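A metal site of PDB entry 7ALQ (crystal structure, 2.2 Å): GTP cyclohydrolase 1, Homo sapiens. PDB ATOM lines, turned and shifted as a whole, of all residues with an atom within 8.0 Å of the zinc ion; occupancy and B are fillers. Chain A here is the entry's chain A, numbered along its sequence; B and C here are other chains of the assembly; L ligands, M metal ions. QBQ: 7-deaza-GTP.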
ATOM      1  N   MET A  99     -23.550  -6.482   5.283  1.00  0.00           N
ATOM      2  CA  MET A  99     -23.097  -5.928   6.557  1.00  0.00           C
ATOM      3  C   MET A  99     -24.134  -6.201   7.606  1.00  0.00           C
ATOM      4  O   MET A  99     -25.298  -5.877   7.354  1.00  0.00           O
ATOM      5  CB  MET A  99     -22.869  -4.435   6.414  1.00  0.00           C
ATOM      6  CG  MET A  99     -21.507  -4.106   5.927  1.00  0.00           C
ATOM      7  SD  MET A  99     -20.459  -3.797   7.341  1.00  0.00           S
ATOM      8  CE  MET A  99     -18.942  -3.654   6.516  1.00  0.00           C
ATOM      9  N   CYS A 100     -23.787  -6.807   8.709  1.00  0.00           N
ATOM     10  CA  CYS A 100     -24.827  -7.056   9.683  1.00  0.00           C
ATOM     11  C   CYS A 100     -25.183  -5.757  10.389  1.00  0.00           C
ATOM     12  O   CYS A 100     -24.328  -4.970  10.742  1.00  0.00           O
ATOM     13  CB  CYS A 100     -24.417  -8.150  10.648  1.00  0.00           C
ATOM     14  SG  CYS A 100     -23.530  -7.556  12.059  1.00  0.00           S
ATOM     15  N   GLU A 101     -26.477  -5.559  10.595  1.00  0.00           N
ATOM     16  CA  GLU A 101     -26.992  -4.344  11.196  1.00  0.00           C
ATOM     17  C   GLU A 101     -26.745  -4.218  12.679  1.00  0.00           C
ATOM     18  O   GLU A 101     -26.782  -3.094  13.189  1.00  0.00           O
ATOM     19  CB  GLU A 101     -28.466  -4.209  10.898  1.00  0.00           C
ATOM     20  CG  GLU A 101     -29.297  -5.264  11.571  1.00  0.00           C
ATOM     21  CD  GLU A 101     -30.767  -5.144  11.254  1.00  0.00           C
ATOM     22  OE1 GLU A 101     -31.598  -5.637  12.062  1.00  0.00           O
ATOM     23  OE2 GLU A 101     -31.103  -4.550  10.193  1.00  0.00           O
ATOM     24  N   HIS A 102     -26.466  -5.337  13.337  1.00  0.00           N
ATOM     25  CA  HIS A 102     -26.212  -5.350  14.760  1.00  0.00           C
ATOM     26  C   HIS A 102     -24.812  -4.934  15.162  1.00  0.00           C
ATOM     27  O   HIS A 102     -24.652  -4.257  16.153  1.00  0.00           O
ATOM     28  CB  HIS A 102     -26.537  -6.729  15.323  1.00  0.00           C
ATOM     29  CG  HIS A 102     -27.964  -7.122  15.165  1.00  0.00           C
ATOM     30  ND1 HIS A 102     -28.379  -8.131  14.324  1.00  0.00           N
ATOM     31  CD2 HIS A 102     -29.099  -6.636  15.731  1.00  0.00           C
ATOM     32  CE1 HIS A 102     -29.686  -8.258  14.382  1.00  0.00           C
ATOM     33  NE2 HIS A 102     -30.153  -7.361  15.231  1.00  0.00           N
ATOM     34  N   HIS A 103     -23.793  -5.299  14.399  1.00  0.00           N
ATOM     35  CA  HIS A 103     -22.417  -4.961  14.766  1.00  0.00           C
ATOM     36  C   HIS A 103     -21.657  -4.163  13.742  1.00  0.00           C
ATOM     37  O   HIS A 103     -20.512  -3.817  13.980  1.00  0.00           O
ATOM     38  CB  HIS A 103     -21.620  -6.223  15.056  1.00  0.00           C
ATOM     39  CG  HIS A 103     -22.113  -6.991  16.240  1.00  0.00           C
ATOM     40  ND1 HIS A 103     -23.112  -7.927  16.150  1.00  0.00           N
ATOM     41  CD2 HIS A 103     -21.721  -6.972  17.532  1.00  0.00           C
ATOM     42  CE1 HIS A 103     -23.328  -8.447  17.352  1.00  0.00           C
ATOM     43  NE2 HIS A 103     -22.490  -7.880  18.205  1.00  0.00           N
ATOM     44  N   LEU A 104     -22.284  -3.896  12.607  1.00  0.00           N
ATOM     45  CA  LEU A 104     -21.673  -3.172  11.512  1.00  0.00           C
ATOM     46  C   LEU A 104     -20.338  -3.770  11.085  1.00  0.00           C
ATOM     47  O   LEU A 104     -19.331  -3.077  11.012  1.00  0.00           O
ATOM     48  CB  LEU A 104     -21.553  -1.682  11.817  1.00  0.00           C
ATOM     49  CG  LEU A 104     -22.894  -0.971  11.960  1.00  0.00           C
ATOM     50  CD1 LEU A 104     -22.716   0.488  12.356  1.00  0.00           C
ATOM     51  CD2 LEU A 104     -23.740  -1.104  10.684  1.00  0.00           C
ATOM     52  N   VAL A 105     -20.344  -5.111  10.896  1.00  0.00           N
ATOM     53  CA  VAL A 105     -19.206  -5.915  10.456  1.00  0.00           C
ATOM     54  C   VAL A 105     -19.736  -6.838   9.367  1.00  0.00           C
ATOM     55  O   VAL A 105     -20.938  -7.179   9.345  1.00  0.00           O
ATOM     56  CB  VAL A 105     -18.499  -6.693  11.596  1.00  0.00           C
ATOM     57  CG1 VAL A 105     -17.911  -5.731  12.627  1.00  0.00           C
ATOM     58  CG2 VAL A 105     -19.449  -7.663  12.282  1.00  0.00           C
ATOM     59  N   PRO A 106     -18.885  -7.230   8.383  1.00  0.00           N
ATOM     60  CA  PRO A 106     -19.397  -8.038   7.274  1.00  0.00           C
ATOM     61  C   PRO A 106     -19.843  -9.459   7.585  1.00  0.00           C
ATOM     62  O   PRO A 106     -19.360 -10.092   8.507  1.00  0.00           O
ATOM     63  CB  PRO A 106     -18.238  -8.061   6.275  1.00  0.00           C
ATOM     64  CG  PRO A 106     -17.273  -6.964   6.738  1.00  0.00           C
ATOM     65  CD  PRO A 106     -17.455  -6.899   8.213  1.00  0.00           C
ATOM     66  N   PHE A 107     -20.823  -9.914   6.813  1.00  0.00           N
ATOM     67  CA  PHE A 107     -21.234 -11.294   6.721  1.00  0.00           C
ATOM     68  C   PHE A 107     -21.159 -11.611   5.253  1.00  0.00           C
ATOM     69  O   PHE A 107     -21.705 -10.892   4.430  1.00  0.00           O
ATOM     70  CB  PHE A 107     -22.528 -11.685   7.462  1.00  0.00           C
ATOM     71  CG  PHE A 107     -23.873 -11.238   6.948  1.00  0.00           C
ATOM     72  CD1 PHE A 107     -24.356  -9.973   7.246  1.00  0.00           C
ATOM     73  CD2 PHE A 107     -24.716 -12.117   6.297  1.00  0.00           C
ATOM     74  CE1 PHE A 107     -25.628  -9.584   6.845  1.00  0.00           C
ATOM     75  CE2 PHE A 107     -25.988 -11.732   5.909  1.00  0.00           C
ATOM     76  CZ  PHE A 107     -26.425 -10.472   6.178  1.00  0.00           C
ATOM     77  N   GLN A 139     -28.141  -5.583   7.118  1.00  0.00           N
ATOM     78  CA  GLN A 139     -29.050  -6.707   7.060  1.00  0.00           C
ATOM     79  C   GLN A 139     -28.921  -7.692   8.216  1.00  0.00           C
ATOM     80  O   GLN A 139     -27.987  -7.616   9.022  1.00  0.00           O
ATOM     81  CB  GLN A 139     -28.724  -7.489   5.764  1.00  0.00           C
ATOM     82  CG  GLN A 139     -29.354  -6.969   4.503  1.00  0.00           C
ATOM     83  CD  GLN A 139     -30.853  -7.114   4.432  1.00  0.00           C
ATOM     84  OE1 GLN A 139     -31.517  -7.502   5.383  1.00  0.00           O
ATOM     85  NE2 GLN A 139     -31.427  -6.789   3.274  1.00  0.00           N
ATOM     86  N   HIS A 169     -20.289 -15.182   9.456  1.00  0.00           N
ATOM     87  CA  HIS A 169     -20.550 -13.929  10.122  1.00  0.00           C
ATOM     88  C   HIS A 169     -19.314 -13.523  10.900  1.00  0.00           C
ATOM     89  O   HIS A 169     -18.925 -14.210  11.813  1.00  0.00           O
ATOM     90  CB  HIS A 169     -21.709 -14.066  11.089  1.00  0.00           C
ATOM     91  CG  HIS A 169     -23.056 -13.993  10.451  1.00  0.00           C
ATOM     92  ND1 HIS A 169     -23.914 -12.945  10.661  1.00  0.00           N
ATOM     93  CD2 HIS A 169     -23.690 -14.841   9.605  1.00  0.00           C
ATOM     94  CE1 HIS A 169     -25.025 -13.141   9.976  1.00  0.00           C
ATOM     95  NE2 HIS A 169     -24.915 -14.284   9.330  1.00  0.00           N
ATOM     96  N   MET A 170     -18.720 -12.380  10.564  1.00  0.00           N
ATOM     97  CA  MET A 170     -17.531 -11.885  11.280  1.00  0.00           C
ATOM     98  C   MET A 170     -17.764 -11.627  12.757  1.00  0.00           C
ATOM     99  O   MET A 170     -16.840 -11.758  13.545  1.00  0.00           O
ATOM    100  CB  MET A 170     -16.989 -10.588  10.642  1.00  0.00           C
ATOM    101  CG  MET A 170     -16.494 -10.756   9.233  1.00  0.00           C
ATOM    102  SD  MET A 170     -15.084 -11.820   9.162  1.00  0.00           S
ATOM    103  CE  MET A 170     -15.759 -13.129   8.182  1.00  0.00           C
ATOM    104  N   CYS A 171     -18.966 -11.221  13.150  1.00  0.00           N
ATOM    105  CA  CYS A 171     -19.287 -10.989  14.538  1.00  0.00           C
ATOM    106  C   CYS A 171     -19.313 -12.268  15.355  1.00  0.00           C
ATOM    107  O   CYS A 171     -19.351 -12.223  16.563  1.00  0.00           O
ATOM    108  CB  CYS A 171     -20.637 -10.285  14.634  1.00  0.00           C
ATOM    109  SG  CYS A 171     -21.946 -11.100  13.706  1.00  0.00           S
ATOM    110  N   MET A 172     -19.300 -13.418  14.686  1.00  0.00           N
ATOM    111  CA  MET A 172     -19.333 -14.710  15.371  1.00  0.00           C
ATOM    112  C   MET A 172     -17.999 -15.424  15.301  1.00  0.00           C
ATOM    113  O   MET A 172     -17.785 -16.415  15.960  1.00  0.00           O
ATOM    114  CB  MET A 172     -20.382 -15.599  14.726  1.00  0.00           C
ATOM    115  CG  MET A 172     -21.767 -15.508  15.316  1.00  0.00           C
ATOM    116  SD  MET A 172     -22.933 -16.573  14.471  1.00  0.00           S
ATOM    117  CE  MET A 172     -22.535 -18.134  15.233  1.00  0.00           C
ATOM    118  N   ARG A 175     -14.962 -12.127  17.053  1.00  0.00           N
ATOM    119  CA  ARG A 175     -15.292 -11.723  18.401  1.00  0.00           C
ATOM    120  C   ARG A 175     -16.459 -12.569  18.899  1.00  0.00           C
ATOM    121  O   ARG A 175     -16.880 -13.495  18.227  1.00  0.00           O
ATOM    122  CB  ARG A 175     -15.732 -10.269  18.399  1.00  0.00           C
ATOM    123  CG  ARG A 175     -16.846  -9.991  17.402  1.00  0.00           C
ATOM    124  CD  ARG A 175     -17.708  -8.816  17.804  1.00  0.00           C
ATOM    125  NE  ARG A 175     -18.209  -8.920  19.166  1.00  0.00           N
ATOM    126  CZ  ARG A 175     -19.349  -9.496  19.502  1.00  0.00           C
ATOM    127  NH1 ARG A 175     -20.117 -10.041  18.579  1.00  0.00           N
ATOM    128  NH2 ARG A 175     -19.712  -9.538  20.766  1.00  0.00           N
ATOM    129  N   ARG B  56     -22.921  -1.723  20.140  1.00  0.00           N
ATOM    130  CA  ARG B  56     -22.409  -3.007  19.718  1.00  0.00           C
ATOM    131  C   ARG B  56     -21.269  -2.802  18.727  1.00  0.00           C
ATOM    132  O   ARG B  56     -20.266  -3.494  18.794  1.00  0.00           O
ATOM    133  CB  ARG B  56     -23.516  -3.885  19.140  1.00  0.00           C
ATOM    134  CG  ARG B  56     -24.393  -4.544  20.174  1.00  0.00           C
ATOM    135  CD  ARG B  56     -25.377  -5.526  19.547  1.00  0.00           C
ATOM    136  NE  ARG B  56     -26.401  -4.848  18.764  1.00  0.00           N
ATOM    137  CZ  ARG B  56     -27.691  -5.120  18.819  1.00  0.00           C
ATOM    138  NH1 ARG B  56     -28.138  -6.073  19.616  1.00  0.00           N
ATOM    139  NH2 ARG B  56     -28.531  -4.445  18.062  1.00  0.00           N
ATOM    140  N   ALA B  60     -17.326  -3.821  19.533  1.00  0.00           N
ATOM    141  CA  ALA B  60     -16.676  -4.715  18.562  1.00  0.00           C
ATOM    142  C   ALA B  60     -15.390  -4.114  18.086  1.00  0.00           C
ATOM    143  O   ALA B  60     -14.379  -4.803  18.148  1.00  0.00           O
ATOM    144  CB  ALA B  60     -17.584  -5.018  17.390  1.00  0.00           C
ATOM    145  N   LEU C 124     -28.351 -15.206  16.158  1.00  0.00           N
ATOM    146  CA  LEU C 124     -27.500 -16.268  15.666  1.00  0.00           C
ATOM    147  C   LEU C 124     -26.457 -16.787  16.653  1.00  0.00           C
ATOM    148  O   LEU C 124     -26.304 -17.990  16.796  1.00  0.00           O
ATOM    149  CB  LEU C 124     -26.831 -15.856  14.350  1.00  0.00           C
ATOM    150  CG  LEU C 124     -27.755 -15.800  13.141  1.00  0.00           C
ATOM    151  CD1 LEU C 124     -26.958 -15.607  11.871  1.00  0.00           C
ATOM    152  CD2 LEU C 124     -28.610 -17.054  13.050  1.00  0.00           C
ATOM    153  N   SER C 125     -25.786 -15.882  17.340  1.00  0.00           N
ATOM    154  CA  SER C 125     -24.764 -16.222  18.326  1.00  0.00           C
ATOM    155  C   SER C 125     -25.274 -17.023  19.506  1.00  0.00           C
ATOM    156  O   SER C 125     -24.534 -17.795  20.090  1.00  0.00           O
ATOM    157  CB  SER C 125     -24.144 -14.944  18.889  1.00  0.00           C
ATOM    158  OG  SER C 125     -22.826 -14.757  18.425  1.00  0.00           O
HETATM  159  O3  QBQ L   1     -27.557  -7.690  21.708  1.00  0.00           O
HETATM  160  C4  QBQ L   1     -26.424 -10.731  14.226  1.00  0.00           C
HETATM  161  C5  QBQ L   1     -27.268 -11.660  16.397  1.00  0.00           C
HETATM  162  O4  QBQ L   1     -25.203  -8.512  21.289  1.00  0.00           O
HETATM  163  C6  QBQ L   1     -27.481 -10.788  18.477  1.00  0.00           C
HETATM  164  N1  QBQ L   1     -29.276 -12.724  14.515  1.00  0.00           N
HETATM  165  C7  QBQ L   1     -27.228  -9.479  19.170  1.00  0.00           C
HETATM  166  C8  QBQ L   1     -26.287 -11.752  18.456  1.00  0.00           C
HETATM  167  N2  QBQ L   1     -27.332 -11.427  14.970  1.00  0.00           N
HETATM  168  C9  QBQ L   1     -25.890 -11.767  16.989  1.00  0.00           C
HETATM  169  O5  QBQ L   1     -22.769  -8.174  21.160  1.00  0.00           O
HETATM  170  C10 QBQ L   1     -28.611 -12.288  11.758  1.00  0.00           C
HETATM  171  O6  QBQ L   1     -23.741  -9.190  23.211  1.00  0.00           O
HETATM  172  N3  QBQ L   1     -29.712 -12.977  12.200  1.00  0.00           N
HETATM  173  O7  QBQ L   1     -23.717 -10.451  21.034  1.00  0.00           O
HETATM  174  O8  QBQ L   1     -21.696 -11.518  22.030  1.00  0.00           O
HETATM  175  N   QBQ L   1     -31.181 -13.757  13.793  1.00  0.00           N
HETATM  176  C   QBQ L   1     -30.019 -13.177  13.519  1.00  0.00           C
HETATM  177  O   QBQ L   1     -27.861 -10.585  17.095  1.00  0.00           O
HETATM  178  C1  QBQ L   1     -28.210 -12.022  14.120  1.00  0.00           C
HETATM  179  C2  QBQ L   1     -27.813 -11.755  12.829  1.00  0.00           C
HETATM  180  C3  QBQ L   1     -26.664 -10.928  12.899  1.00  0.00           C
HETATM  181  O1  QBQ L   1     -27.130  -9.793  20.565  1.00  0.00           O
HETATM  182  O10 QBQ L   1     -22.103 -11.682  19.680  1.00  0.00           O
HETATM  183  O11 QBQ L   1     -26.719 -13.031  18.891  1.00  0.00           O
HETATM  184  O12 QBQ L   1     -25.286 -12.965  16.541  1.00  0.00           O
HETATM  185  O13 QBQ L   1     -28.369 -12.194  10.571  1.00  0.00           O
HETATM  186  O2  QBQ L   1     -26.653  -9.626  22.935  1.00  0.00           O
HETATM  187  O9  QBQ L   1     -23.467 -12.836  21.228  1.00  0.00           O
HETATM  188  P   QBQ L   1     -26.697  -8.863  21.687  1.00  0.00           P
HETATM  189  P1  QBQ L   1     -23.788  -9.047  21.777  1.00  0.00           P
HETATM  190  P2  QBQ L   1     -22.688 -11.659  20.937  1.00  0.00           P
HETATM  191 ZN    ZN M   1     -23.271  -8.999  14.092  1.00  0.00          ZN
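An oxygen (O10) of the ligand lies within hydrogen-bond range of the side-chain hydroxyl of Ser 125 of chain C, 3.4 Å away.
An oxygen (O10) of the ligand is in salt-bridge range of the guanidinium group (NH1) of Arg 175, at 2.8 Å.
O12 of the ligand is in hydrogen-bond range of N of Ser 125 of chain C (3.1 Å).
O3 of the ligand lies within salt-bridge range of NH1 of Arg 56 of chain B (2.7 Å).
The backbone NH (N) of Leu 124 of chain C lies within hydrogen-bond range of a nitrogen (N1) of the ligand (3.1 Å).
O5 of the ligand is in hydrogen-bond range of NE2 of His 103, 3.0 Å away.
Of the 19 residues printed, 3 come within 4 Å of the zinc ion.
A ring nitrogen (ND1) of His 103 is bound to the zinc ion (2.3 Å).
SG of Cys 100 binds the zinc ion, 2.5 Å away.
The zinc ion is bound by SG of Cys 171, at 2.5 Å.
The zinc ion has three donor atoms within binding distance.
The backbone NH (N) of Cys 100 sits at hydrogen-bond distance from the backbone carbonyl oxygen (O) of Val 105.
The guanidinium group (NH1) of Arg 175 is in hydrogen-bond range of a ring nitrogen (NE2) of His 103, at 3.2 Å.
NH1 of Arg 175 sits at hydrogen-bond distance from O of Cys 171 (3.1 Å).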
